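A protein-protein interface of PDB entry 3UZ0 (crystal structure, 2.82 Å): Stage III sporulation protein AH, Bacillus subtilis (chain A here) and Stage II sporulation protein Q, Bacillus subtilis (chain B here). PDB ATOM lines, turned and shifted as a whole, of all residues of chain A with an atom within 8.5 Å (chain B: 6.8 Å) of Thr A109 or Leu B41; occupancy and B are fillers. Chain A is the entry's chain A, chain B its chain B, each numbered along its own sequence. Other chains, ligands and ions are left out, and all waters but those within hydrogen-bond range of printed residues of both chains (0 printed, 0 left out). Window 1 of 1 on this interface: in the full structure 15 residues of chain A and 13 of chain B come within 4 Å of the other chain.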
ATOM      1  N   GLN A  80     -12.660 -14.760 -17.468  1.00  0.00           N
ATOM      2  CA  GLN A  80     -12.298 -14.556 -18.868  1.00  0.00           C
ATOM      3  C   GLN A  80     -12.726 -15.797 -19.628  1.00  0.00           C
ATOM      4  O   GLN A  80     -12.046 -16.805 -19.563  1.00  0.00           O
ATOM      5  CB  GLN A  80     -10.784 -14.410 -18.953  1.00  0.00           C
ATOM      6  CG  GLN A  80     -10.057 -15.465 -18.109  1.00  0.00           C
ATOM      7  CD  GLN A  80      -8.613 -15.129 -17.813  1.00  0.00           C
ATOM      8  OE1 GLN A  80      -7.699 -15.898 -18.144  1.00  0.00           O
ATOM      9  NE2 GLN A  80      -8.394 -13.990 -17.155  1.00  0.00           N
ATOM     10  N   TYR A  82     -14.301 -19.325 -20.398  1.00  0.00           N
ATOM     11  CA  TYR A  82     -14.305 -20.483 -19.481  1.00  0.00           C
ATOM     12  C   TYR A  82     -15.594 -20.721 -18.687  1.00  0.00           C
ATOM     13  O   TYR A  82     -15.766 -20.215 -17.578  1.00  0.00           O
ATOM     14  CB  TYR A  82     -13.061 -20.514 -18.581  1.00  0.00           C
ATOM     15  CG  TYR A  82     -11.792 -20.312 -19.349  1.00  0.00           C
ATOM     16  CD1 TYR A  82     -11.495 -21.085 -20.474  1.00  0.00           C
ATOM     17  CD2 TYR A  82     -10.907 -19.319 -18.983  1.00  0.00           C
ATOM     18  CE1 TYR A  82     -10.319 -20.871 -21.204  1.00  0.00           C
ATOM     19  CE2 TYR A  82      -9.755 -19.094 -19.696  1.00  0.00           C
ATOM     20  CZ  TYR A  82      -9.459 -19.867 -20.801  1.00  0.00           C
ATOM     21  OH  TYR A  82      -8.287 -19.607 -21.469  1.00  0.00           O
ATOM     22  N   SER A 104      -4.358 -22.912 -26.032  1.00  0.00           N
ATOM     23  CA  SER A 104      -3.109 -22.360 -26.542  1.00  0.00           C
ATOM     24  C   SER A 104      -2.165 -21.934 -25.433  1.00  0.00           C
ATOM     25  O   SER A 104      -2.597 -21.660 -24.320  1.00  0.00           O
ATOM     26  CB  SER A 104      -3.399 -21.136 -27.409  1.00  0.00           C
ATOM     27  OG  SER A 104      -3.954 -20.080 -26.648  1.00  0.00           O
ATOM     28  N   LYS A 105      -0.881 -21.834 -25.768  1.00  0.00           N
ATOM     29  CA  LYS A 105       0.138 -21.267 -24.889  1.00  0.00           C
ATOM     30  C   LYS A 105      -0.306 -19.904 -24.388  1.00  0.00           C
ATOM     31  O   LYS A 105       0.073 -19.464 -23.305  1.00  0.00           O
ATOM     32  CB  LYS A 105       1.479 -21.139 -25.636  1.00  0.00           C
ATOM     33  CG  LYS A 105       2.175 -22.486 -25.851  1.00  0.00           C
ATOM     34  CD  LYS A 105       3.213 -22.508 -26.978  1.00  0.00           C
ATOM     35  CE  LYS A 105       3.717 -23.952 -27.186  1.00  0.00           C
ATOM     36  NZ  LYS A 105       4.697 -24.152 -28.303  1.00  0.00           N
ATOM     37  N   SER A 106      -1.118 -19.238 -25.191  1.00  0.00           N
ATOM     38  CA  SER A 106      -1.584 -17.902 -24.876  1.00  0.00           C
ATOM     39  C   SER A 106      -2.549 -17.988 -23.709  1.00  0.00           C
ATOM     40  O   SER A 106      -2.415 -17.275 -22.713  1.00  0.00           O
ATOM     41  CB  SER A 106      -2.270 -17.292 -26.106  1.00  0.00           C
ATOM     42  OG  SER A 106      -3.146 -16.237 -25.751  1.00  0.00           O
ATOM     43  N   LYS A 107      -3.521 -18.877 -23.839  1.00  0.00           N
ATOM     44  CA  LYS A 107      -4.558 -19.004 -22.837  1.00  0.00           C
ATOM     45  C   LYS A 107      -3.950 -19.404 -21.504  1.00  0.00           C
ATOM     46  O   LYS A 107      -4.275 -18.828 -20.460  1.00  0.00           O
ATOM     47  CB  LYS A 107      -5.618 -20.014 -23.289  1.00  0.00           C
ATOM     48  CG  LYS A 107      -6.435 -19.550 -24.500  1.00  0.00           C
ATOM     49  CD  LYS A 107      -7.887 -20.055 -24.461  1.00  0.00           C
ATOM     50  CE  LYS A 107      -8.645 -19.788 -25.766  1.00  0.00           C
ATOM     51  NZ  LYS A 107      -8.792 -18.338 -26.134  1.00  0.00           N
ATOM     52  N   ALA A 108      -3.051 -20.380 -21.561  1.00  0.00           N
ATOM     53  CA  ALA A 108      -2.432 -20.951 -20.374  1.00  0.00           C
ATOM     54  C   ALA A 108      -1.752 -19.896 -19.525  1.00  0.00           C
ATOM     55  O   ALA A 108      -1.906 -19.869 -18.303  1.00  0.00           O
ATOM     56  CB  ALA A 108      -1.442 -22.027 -20.766  1.00  0.00           C
ATOM     57  N   THR A 109      -0.987 -19.032 -20.175  1.00  0.00           N
ATOM     58  CA  THR A 109      -0.319 -17.956 -19.477  1.00  0.00           C
ATOM     59  C   THR A 109      -1.288 -17.007 -18.769  1.00  0.00           C
ATOM     60  O   THR A 109      -1.073 -16.638 -17.625  1.00  0.00           O
ATOM     61  CB  THR A 109       0.532 -17.179 -20.442  1.00  0.00           C
ATOM     62  OG1 THR A 109       1.606 -18.021 -20.856  1.00  0.00           O
ATOM     63  CG2 THR A 109       1.096 -15.935 -19.782  1.00  0.00           C
ATOM     64  N   ALA A 110      -2.358 -16.614 -19.440  1.00  0.00           N
ATOM     65  CA  ALA A 110      -3.355 -15.759 -18.815  1.00  0.00           C
ATOM     66  C   ALA A 110      -3.821 -16.360 -17.507  1.00  0.00           C
ATOM     67  O   ALA A 110      -4.161 -15.646 -16.568  1.00  0.00           O
ATOM     68  CB  ALA A 110      -4.528 -15.590 -19.725  1.00  0.00           C
ATOM     69  N   ILE A 111      -3.859 -17.685 -17.470  1.00  0.00           N
ATOM     70  CA  ILE A 111      -4.343 -18.420 -16.311  1.00  0.00           C
ATOM     71  C   ILE A 111      -3.274 -18.542 -15.238  1.00  0.00           C
ATOM     72  O   ILE A 111      -3.495 -18.213 -14.078  1.00  0.00           O
ATOM     73  CB  ILE A 111      -4.878 -19.779 -16.689  1.00  0.00           C
ATOM     74  CG1 ILE A 111      -6.255 -19.621 -17.319  1.00  0.00           C
ATOM     75  CG2 ILE A 111      -4.976 -20.652 -15.471  1.00  0.00           C
ATOM     76  CD1 ILE A 111      -6.790 -20.911 -17.862  1.00  0.00           C
ATOM     77  N   ILE A 112      -2.145 -19.108 -15.620  1.00  0.00           N
ATOM     78  CA  ILE A 112      -0.960 -19.080 -14.793  1.00  0.00           C
ATOM     79  C   ILE A 112      -0.655 -17.688 -14.229  1.00  0.00           C
ATOM     80  O   ILE A 112      -0.377 -17.546 -13.041  1.00  0.00           O
ATOM     81  CB  ILE A 112       0.247 -19.552 -15.608  1.00  0.00           C
ATOM     82  CG1 ILE A 112       0.066 -21.010 -16.000  1.00  0.00           C
ATOM     83  CG2 ILE A 112       1.510 -19.386 -14.817  1.00  0.00           C
ATOM     84  CD1 ILE A 112       1.115 -21.486 -16.920  1.00  0.00           C
ATOM     85  N   ASP A 113      -0.703 -16.665 -15.078  1.00  0.00           N
ATOM     86  CA  ASP A 113      -0.417 -15.291 -14.651  1.00  0.00           C
ATOM     87  C   ASP A 113      -1.183 -14.904 -13.404  1.00  0.00           C
ATOM     88  O   ASP A 113      -0.633 -14.271 -12.503  1.00  0.00           O
ATOM     89  CB  ASP A 113      -0.760 -14.288 -15.752  1.00  0.00           C
ATOM     90  CG  ASP A 113       0.455 -13.865 -16.551  1.00  0.00           C
ATOM     91  OD1 ASP A 113       1.575 -14.261 -16.153  1.00  0.00           O
ATOM     92  OD2 ASP A 113       0.293 -13.134 -17.563  1.00  0.00           O
ATOM     93  N   LEU A 114      -2.459 -15.264 -13.350  1.00  0.00           N
ATOM     94  CA  LEU A 114      -3.267 -14.795 -12.248  1.00  0.00           C
ATOM     95  C   LEU A 114      -3.208 -15.718 -11.048  1.00  0.00           C
ATOM     96  O   LEU A 114      -3.591 -15.336  -9.948  1.00  0.00           O
ATOM     97  CB  LEU A 114      -4.699 -14.462 -12.688  1.00  0.00           C
ATOM     98  CG  LEU A 114      -5.725 -15.519 -13.047  1.00  0.00           C
ATOM     99  CD1 LEU A 114      -6.176 -16.240 -11.803  1.00  0.00           C
ATOM    100  CD2 LEU A 114      -6.900 -14.838 -13.718  1.00  0.00           C
ATOM    101  N   VAL A 115      -2.687 -16.920 -11.243  1.00  0.00           N
ATOM    102  CA  VAL A 115      -2.434 -17.793 -10.104  1.00  0.00           C
ATOM    103  C   VAL A 115      -1.207 -17.303  -9.369  1.00  0.00           C
ATOM    104  O   VAL A 115      -1.180 -17.275  -8.143  1.00  0.00           O
ATOM    105  CB  VAL A 115      -2.193 -19.233 -10.508  1.00  0.00           C
ATOM    106  CG1 VAL A 115      -2.027 -20.080  -9.268  1.00  0.00           C
ATOM    107  CG2 VAL A 115      -3.349 -19.740 -11.338  1.00  0.00           C
ATOM    108  N   ALA A 116      -0.192 -16.919 -10.131  1.00  0.00           N
ATOM    109  CA  ALA A 116       0.994 -16.309  -9.568  1.00  0.00           C
ATOM    110  C   ALA A 116       0.605 -15.104  -8.720  1.00  0.00           C
ATOM    111  O   ALA A 116       1.044 -14.953  -7.581  1.00  0.00           O
ATOM    112  CB  ALA A 116       1.911 -15.873 -10.671  1.00  0.00           C
ATOM    113  N   ASP A 124       4.916 -25.346  -9.136  1.00  0.00           N
ATOM    114  CA  ASP A 124       4.504 -25.588 -10.516  1.00  0.00           C
ATOM    115  C   ASP A 124       2.994 -25.344 -10.693  1.00  0.00           C
ATOM    116  O   ASP A 124       2.229 -25.378  -9.722  1.00  0.00           O
ATOM    117  CB  ASP A 124       4.880 -27.017 -10.914  1.00  0.00           C
ATOM    118  CG  ASP A 124       4.802 -27.262 -12.421  1.00  0.00           C
ATOM    119  OD1 ASP A 124       4.574 -26.302 -13.193  1.00  0.00           O
ATOM    120  OD2 ASP A 124       4.995 -28.428 -12.833  1.00  0.00           O
ATOM    121  N   VAL A 125       2.565 -25.074 -11.923  1.00  0.00           N
ATOM    122  CA  VAL A 125       1.135 -24.975 -12.222  1.00  0.00           C
ATOM    123  C   VAL A 125       0.801 -25.770 -13.453  1.00  0.00           C
ATOM    124  O   VAL A 125       1.524 -25.706 -14.439  1.00  0.00           O
ATOM    125  CB  VAL A 125       0.704 -23.545 -12.517  1.00  0.00           C
ATOM    126  CG1 VAL A 125      -0.796 -23.508 -12.804  1.00  0.00           C
ATOM    127  CG2 VAL A 125       1.065 -22.629 -11.364  1.00  0.00           C
ATOM    128  N   ALA A 126      -0.281 -26.532 -13.413  1.00  0.00           N
ATOM    129  CA  ALA A 126      -0.644 -27.301 -14.596  1.00  0.00           C
ATOM    130  C   ALA A 126      -2.092 -27.110 -14.990  1.00  0.00           C
ATOM    131  O   ALA A 126      -2.999 -27.637 -14.343  1.00  0.00           O
ATOM    132  CB  ALA A 126      -0.354 -28.757 -14.382  1.00  0.00           C
ATOM    133  N   VAL A 127      -2.276 -26.420 -16.116  1.00  0.00           N
ATOM    134  CA  VAL A 127      -3.580 -26.097 -16.685  1.00  0.00           C
ATOM    135  C   VAL A 127      -3.927 -27.105 -17.772  1.00  0.00           C
ATOM    136  O   VAL A 127      -3.173 -27.284 -18.724  1.00  0.00           O
ATOM    137  CB  VAL A 127      -3.515 -24.750 -17.366  1.00  0.00           C
ATOM    138  CG1 VAL A 127      -4.864 -24.159 -17.461  1.00  0.00           C
ATOM    139  CG2 VAL A 127      -2.606 -23.838 -16.600  1.00  0.00           C
ATOM    140  N   PHE A 129      -6.955 -27.934 -20.537  1.00  0.00           N
ATOM    141  CA  PHE A 129      -8.186 -27.419 -21.137  1.00  0.00           C
ATOM    142  C   PHE A 129      -8.961 -28.598 -21.656  1.00  0.00           C
ATOM    143  O   PHE A 129      -8.649 -29.144 -22.709  1.00  0.00           O
ATOM    144  CB  PHE A 129      -7.896 -26.514 -22.327  1.00  0.00           C
ATOM    145  CG  PHE A 129      -7.022 -25.351 -22.015  1.00  0.00           C
ATOM    146  CD1 PHE A 129      -7.527 -24.066 -22.035  1.00  0.00           C
ATOM    147  CD2 PHE A 129      -5.687 -25.529 -21.739  1.00  0.00           C
ATOM    148  CE1 PHE A 129      -6.713 -22.970 -21.759  1.00  0.00           C
ATOM    149  CE2 PHE A 129      -4.880 -24.445 -21.456  1.00  0.00           C
ATOM    150  CZ  PHE A 129      -5.399 -23.163 -21.466  1.00  0.00           C
ATOM    151  N   LYS B  25      14.696 -24.041 -24.520  1.00  0.00           N
ATOM    152  CA  LYS B  25      13.600 -23.677 -23.624  1.00  0.00           C
ATOM    153  C   LYS B  25      14.163 -23.124 -22.318  1.00  0.00           C
ATOM    154  O   LYS B  25      15.095 -23.678 -21.757  1.00  0.00           O
ATOM    155  CB  LYS B  25      12.673 -24.873 -23.376  1.00  0.00           C
ATOM    156  CG  LYS B  25      11.309 -24.486 -22.805  1.00  0.00           C
ATOM    157  CD  LYS B  25      10.319 -25.667 -22.713  1.00  0.00           C
ATOM    158  CE  LYS B  25       9.532 -25.909 -24.009  1.00  0.00           C
ATOM    159  NZ  LYS B  25       8.698 -24.742 -24.462  1.00  0.00           N
ATOM    160  N   LYS B  26      13.594 -22.028 -21.833  1.00  0.00           N
ATOM    161  CA  LYS B  26      14.119 -21.395 -20.625  1.00  0.00           C
ATOM    162  C   LYS B  26      13.308 -21.726 -19.373  1.00  0.00           C
ATOM    163  O   LYS B  26      12.260 -22.368 -19.443  1.00  0.00           O
ATOM    164  CB  LYS B  26      14.202 -19.881 -20.827  1.00  0.00           C
ATOM    165  CG  LYS B  26      15.122 -19.486 -21.978  1.00  0.00           C
ATOM    166  CD  LYS B  26      15.250 -17.978 -22.143  1.00  0.00           C
ATOM    167  CE  LYS B  26      16.502 -17.602 -22.942  1.00  0.00           C
ATOM    168  NZ  LYS B  26      16.754 -16.131 -22.973  1.00  0.00           N
ATOM    169  N   TYR B  28      10.820 -20.876 -16.537  1.00  0.00           N
ATOM    170  CA  TYR B  28       9.695 -19.944 -16.593  1.00  0.00           C
ATOM    171  C   TYR B  28       9.768 -18.897 -15.469  1.00  0.00           C
ATOM    172  O   TYR B  28       9.877 -19.224 -14.291  1.00  0.00           O
ATOM    173  CB  TYR B  28       8.370 -20.714 -16.586  1.00  0.00           C
ATOM    174  CG  TYR B  28       7.126 -19.850 -16.591  1.00  0.00           C
ATOM    175  CD1 TYR B  28       6.684 -19.243 -15.420  1.00  0.00           C
ATOM    176  CD2 TYR B  28       6.361 -19.679 -17.752  1.00  0.00           C
ATOM    177  CE1 TYR B  28       5.549 -18.460 -15.396  1.00  0.00           C
ATOM    178  CE2 TYR B  28       5.199 -18.882 -17.737  1.00  0.00           C
ATOM    179  CZ  TYR B  28       4.811 -18.278 -16.549  1.00  0.00           C
ATOM    180  OH  TYR B  28       3.690 -17.488 -16.480  1.00  0.00           O
ATOM    181  N   LYS B  34       5.641 -11.482 -21.611  1.00  0.00           N
ATOM    182  CA  LYS B  34       4.837 -12.618 -21.993  1.00  0.00           C
ATOM    183  C   LYS B  34       5.450 -13.085 -23.302  1.00  0.00           C
ATOM    184  O   LYS B  34       6.398 -12.483 -23.792  1.00  0.00           O
ATOM    185  CB  LYS B  34       3.363 -12.242 -22.139  1.00  0.00           C
ATOM    186  CG  LYS B  34       3.026 -11.366 -23.327  1.00  0.00           C
ATOM    187  CD  LYS B  34       1.590 -10.834 -23.224  1.00  0.00           C
ATOM    188  CE  LYS B  34       0.571 -11.960 -23.113  1.00  0.00           C
ATOM    189  NZ  LYS B  34       0.590 -12.845 -24.314  1.00  0.00           N
ATOM    190  N   GLU B  35       4.959 -14.191 -23.828  1.00  0.00           N
ATOM    191  CA  GLU B  35       5.467 -14.739 -25.076  1.00  0.00           C
ATOM    192  C   GLU B  35       6.874 -15.313 -24.908  1.00  0.00           C
ATOM    193  O   GLU B  35       7.311 -16.148 -25.709  1.00  0.00           O
ATOM    194  CB  GLU B  35       5.469 -13.675 -26.174  1.00  0.00           C
ATOM    195  CG  GLU B  35       6.855 -13.162 -26.534  1.00  0.00           C
ATOM    196  CD  GLU B  35       6.903 -11.648 -26.627  1.00  0.00           C
ATOM    197  OE1 GLU B  35       7.921 -11.111 -27.116  1.00  0.00           O
ATOM    198  OE2 GLU B  35       5.921 -10.994 -26.206  1.00  0.00           O
ATOM    199  N   GLU B  36       7.593 -14.871 -23.879  1.00  0.00           N
ATOM    200  CA  GLU B  36       8.745 -15.633 -23.439  1.00  0.00           C
ATOM    201  C   GLU B  36       8.341 -16.466 -22.238  1.00  0.00           C
ATOM    202  O   GLU B  36       9.036 -17.419 -21.867  1.00  0.00           O
ATOM    203  CB  GLU B  36       9.939 -14.729 -23.139  1.00  0.00           C
ATOM    204  CG  GLU B  36       9.891 -14.015 -21.805  1.00  0.00           C
ATOM    205  CD  GLU B  36      10.838 -12.826 -21.764  1.00  0.00           C
ATOM    206  OE1 GLU B  36      11.284 -12.432 -20.660  1.00  0.00           O
ATOM    207  OE2 GLU B  36      11.129 -12.281 -22.854  1.00  0.00           O
ATOM    208  N   LYS B  37       7.194 -16.117 -21.657  1.00  0.00           N
ATOM    209  CA  LYS B  37       6.534 -16.974 -20.695  1.00  0.00           C
ATOM    210  C   LYS B  37       5.948 -18.090 -21.525  1.00  0.00           C
ATOM    211  O   LYS B  37       6.156 -19.270 -21.255  1.00  0.00           O
ATOM    212  CB  LYS B  37       5.399 -16.240 -19.998  1.00  0.00           C
ATOM    213  CG  LYS B  37       5.829 -15.285 -18.904  1.00  0.00           C
ATOM    214  CD  LYS B  37       4.666 -14.372 -18.519  1.00  0.00           C
ATOM    215  CE  LYS B  37       4.942 -13.600 -17.244  1.00  0.00           C
ATOM    216  NZ  LYS B  37       3.792 -12.718 -16.912  1.00  0.00           N
ATOM    217  N   GLU B  38       5.227 -17.699 -22.565  1.00  0.00           N
ATOM    218  CA  GLU B  38       4.620 -18.654 -23.469  1.00  0.00           C
ATOM    219  C   GLU B  38       5.642 -19.670 -24.015  1.00  0.00           C
ATOM    220  O   GLU B  38       5.318 -20.838 -24.276  1.00  0.00           O
ATOM    221  CB  GLU B  38       3.908 -17.895 -24.582  1.00  0.00           C
ATOM    222  CG  GLU B  38       2.961 -16.840 -24.032  1.00  0.00           C
ATOM    223  CD  GLU B  38       2.141 -16.142 -25.111  1.00  0.00           C
ATOM    224  OE1 GLU B  38       2.397 -16.384 -26.315  1.00  0.00           O
ATOM    225  OE2 GLU B  38       1.233 -15.351 -24.751  1.00  0.00           O
ATOM    226  N   ALA B  39       6.886 -19.233 -24.156  1.00  0.00           N
ATOM    227  CA  ALA B  39       7.935 -20.113 -24.641  1.00  0.00           C
ATOM    228  C   ALA B  39       8.633 -20.856 -23.500  1.00  0.00           C
ATOM    229  O   ALA B  39       9.587 -21.602 -23.727  1.00  0.00           O
ATOM    230  CB  ALA B  39       8.934 -19.324 -25.449  1.00  0.00           C
ATOM    231  N   ALA B  40       8.198 -20.583 -22.269  1.00  0.00           N
ATOM    232  CA  ALA B  40       8.632 -21.328 -21.088  1.00  0.00           C
ATOM    233  C   ALA B  40       7.624 -22.378 -20.623  1.00  0.00           C
ATOM    234  O   ALA B  40       7.795 -22.968 -19.560  1.00  0.00           O
ATOM    235  CB  ALA B  40       9.001 -20.405 -19.965  1.00  0.00           C
ATOM    236  N   LEU B  41       6.547 -22.566 -21.382  1.00  0.00           N
ATOM    237  CA  LEU B  41       5.576 -23.618 -21.072  1.00  0.00           C
ATOM    238  C   LEU B  41       6.021 -24.954 -21.633  1.00  0.00           C
ATOM    239  O   LEU B  41       6.564 -25.015 -22.730  1.00  0.00           O
ATOM    240  CB  LEU B  41       4.191 -23.279 -21.624  1.00  0.00           C
ATOM    241  CG  LEU B  41       3.267 -22.328 -20.849  1.00  0.00           C
ATOM    242  CD1 LEU B  41       3.673 -22.194 -19.374  1.00  0.00           C
ATOM    243  CD2 LEU B  41       3.231 -20.976 -21.496  1.00  0.00           C
ATOM    244  N   VAL B  42       5.800 -26.021 -20.872  1.00  0.00           N
ATOM    245  CA  VAL B  42       5.978 -27.373 -21.383  1.00  0.00           C
ATOM    246  C   VAL B  42       4.590 -27.959 -21.543  1.00  0.00           C
ATOM    247  O   VAL B  42       3.695 -27.634 -20.781  1.00  0.00           O
ATOM    248  CB  VAL B  42       6.794 -28.254 -20.437  1.00  0.00           C
ATOM    249  CG1 VAL B  42       7.995 -27.500 -19.925  1.00  0.00           C
ATOM    250  CG2 VAL B  42       5.944 -28.712 -19.285  1.00  0.00           C
ATOM    251  N   THR B  43       4.384 -28.792 -22.553  1.00  0.00           N
ATOM    252  CA  THR B  43       3.021 -29.225 -22.861  1.00  0.00           C
ATOM    253  C   THR B  43       2.922 -30.613 -23.465  1.00  0.00           C
ATOM    254  O   THR B  43       3.852 -31.093 -24.125  1.00  0.00           O
ATOM    255  CB  THR B  43       2.325 -28.253 -23.818  1.00  0.00           C
ATOM    256  OG1 THR B  43       1.032 -28.770 -24.153  1.00  0.00           O
ATOM    257  CG2 THR B  43       3.149 -28.103 -25.085  1.00  0.00           C
ATOM    258  N   TYR B  48      -0.789 -27.841 -20.151  1.00  0.00           N
ATOM    259  CA  TYR B  48       0.386 -26.983 -20.144  1.00  0.00           C
ATOM    260  C   TYR B  48       0.903 -26.777 -18.725  1.00  0.00           C
ATOM    261  O   TYR B  48       0.126 -26.637 -17.773  1.00  0.00           O
ATOM    262  CB  TYR B  48       0.009 -25.621 -20.668  1.00  0.00           C
ATOM    263  CG  TYR B  48      -0.505 -25.579 -22.078  1.00  0.00           C
ATOM    264  CD1 TYR B  48       0.305 -25.129 -23.119  1.00  0.00           C
ATOM    265  CD2 TYR B  48      -1.801 -25.946 -22.369  1.00  0.00           C
ATOM    266  CE1 TYR B  48      -0.158 -25.061 -24.400  1.00  0.00           C
ATOM    267  CE2 TYR B  48      -2.280 -25.883 -23.664  1.00  0.00           C
ATOM    268  CZ  TYR B  48      -1.453 -25.438 -24.673  1.00  0.00           C
ATOM    269  OH  TYR B  48      -1.935 -25.368 -25.958  1.00  0.00           O
ATOM    270  N   SER B  49       2.218 -26.718 -18.590  1.00  0.00           N
ATOM    271  CA  SER B  49       2.854 -26.652 -17.288  1.00  0.00           C
ATOM    272  C   SER B  49       4.081 -25.723 -17.370  1.00  0.00           C
ATOM    273  O   SER B  49       4.442 -25.263 -18.457  1.00  0.00           O
ATOM    274  CB  SER B  49       3.222 -28.081 -16.869  1.00  0.00           C
ATOM    275  OG  SER B  49       4.540 -28.174 -16.349  1.00  0.00           O
ATOM    276  N   LEU B  50       4.735 -25.438 -16.246  1.00  0.00           N
ATOM    277  CA  LEU B  50       5.895 -24.545 -16.294  1.00  0.00           C
ATOM    278  C   LEU B  50       7.158 -25.327 -16.554  1.00  0.00           C
ATOM    279  O   LEU B  50       7.327 -26.445 -16.065  1.00  0.00           O
ATOM    280  CB  LEU B  50       6.076 -23.798 -14.987  1.00  0.00           C
ATOM    281  CG  LEU B  50       4.874 -23.154 -14.324  1.00  0.00           C
ATOM    282  CD1 LEU B  50       5.376 -22.320 -13.159  1.00  0.00           C
ATOM    283  CD2 LEU B  50       4.173 -22.312 -15.332  1.00  0.00           C
ATOM    284  N   SER B  51       8.051 -24.747 -17.331  1.00  0.00           N
ATOM    285  CA  SER B  51       9.381 -25.313 -17.439  1.00  0.00           C
ATOM    286  C   SER B  51      10.109 -24.967 -16.150  1.00  0.00           C
ATOM    287  O   SER B  51      10.232 -23.798 -15.782  1.00  0.00           O
ATOM    288  CB  SER B  51      10.131 -24.751 -18.646  1.00  0.00           C
ATOM    289  OG  SER B  51      11.522 -24.899 -18.468  1.00  0.00           O
ATOM    290  N   GLU B 129       8.601 -31.420 -27.987  1.00  0.00           N
ATOM    291  CA  GLU B 129       7.836 -30.896 -29.091  1.00  0.00           C
ATOM    292  C   GLU B 129       8.773 -31.149 -30.257  1.00  0.00           C
ATOM    293  O   GLU B 129       9.922 -31.557 -30.046  1.00  0.00           O
ATOM    294  CB  GLU B 129       7.547 -29.413 -28.884  1.00  0.00           C
ATOM    295  CG  GLU B 129       6.886 -29.110 -27.537  1.00  0.00           C
ATOM    296  CD  GLU B 129       7.149 -27.687 -27.038  1.00  0.00           C
ATOM    297  OE1 GLU B 129       7.288 -26.770 -27.879  1.00  0.00           O
ATOM    298  OE2 GLU B 129       7.221 -27.490 -25.800  1.00  0.00           O
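The side-chain carboxylate (OE1) of Glu B129 is in salt-bridge range of the side-chain amino group (NZ) of Lys A105 (3.7 Å).
The backbone NH of Ser A104 lies close to the side-chain hydroxyl of Tyr B48, at 3.5 Å.
O of Val A127 sits at hydrogen-bond distance from N of Tyr B48, 2.8 Å away.
OD1 of Asp A124 is in hydrogen-bond range of N of Leu B50.
NZ of Lys B37 lies within salt-bridge range of OD1 of Asp A113 (2.8 Å).
The side-chain hydroxyl (OG) of Ser A104 sits close to the backbone NH (N) of Ser A106 (3.3 Å).
The side-chain carboxylate of Glu B129 is in salt-bridge range of the side-chain amino group of Lys B25 (3.4 Å).
OE2 of Glu B38 lies within salt-bridge range of NZ of Lys B34, at 2.6 Å.
The side-chain hydroxyl (OG) of Ser A104 lies within hydrogen-bond range of the backbone NH (N) of Lys A107.
The backbone carbonyl oxygen of Val B42 is in hydrogen-bond range of the backbone NH of Ser B49, 2.8 Å away.
The backbone NH (N) of Tyr B28 lies within hydrogen-bond range of the backbone carbonyl oxygen (O) of Ser B51, 3.1 Å away.
Among the printed residues, merely in contact across the chains: Lys A105 with Glu B38 (3.8 Å), Lys A105 with Leu B41 (3.9 Å), Lys A105 with Tyr B48 (3.6 Å), Ser A106 with Glu B38 (3.8 Å), Ala A108 with Tyr B48 (3.9 Å), Thr A109 with Glu B38 (3.6 Å), Thr A109 with Leu B41 (3.4 Å), Ile A112 with Tyr B28 (3.3 Å), Ile A112 with Leu B41 (3.6 Å), Ile A112 with Leu B50 (3.5 Å), Asp A113 with Tyr B28 (3.9 Å), Asp A124 with Ser B49 (3.6 Å), Val A125 with Tyr B48 (3.7 Å), Val A125 with Ser B49 (3.3 Å), Val A125 with Leu B50 (3.7 Å), Ala A126 with Tyr B48 (3.3 Å) and Phe A129 with Tyr B48 (3.5 Å).
Of the printed residues of chain B, Ile A112 touches Tyr B28, Leu B41 and Leu B50.
Printed residues of chain B within 4 Å of Val A125: Tyr B48, Ser B49 and Leu B50.
Of the printed residues of chain A, Tyr B28 touches Ile A112 and Asp A113.
No residue of chain A comes within 4 Å of Ala B40.
Of chain A, only Lys A105 (3.9 Å), Thr A109 (3.4 Å) and Ile A112 (3.6 Å) come within 4 Å of Leu B41.
No residue of chain A comes within 4 Å of Val B42.
Printed residues of chain A within 4 Å of Glu B129: Lys A105 (3.7 Å).
The nearest residue of chain A that does not touch Leu B41 is Ala A108 (4.7 Å).
Hydrophobic or aromatic side chains of chain B within 4 Å of the printed part of chain A: Tyr B28, Leu B41, Tyr B48 and Leu B50.
Hydrophobic or aromatic side chains of chain A that line the printed part of chain B: Ala A108, Ile A112 and Phe A129.
Among the printed residues, 22 pairs touch across the chains.
Among the printed residues, Asp or Glu carboxylates within 4 Å of a Lys or Arg side-chain nitrogen of the other chain: Lys A105 with Glu B129 (3.7 Å) and Asp A113 with Lys B37 (2.8 Å).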
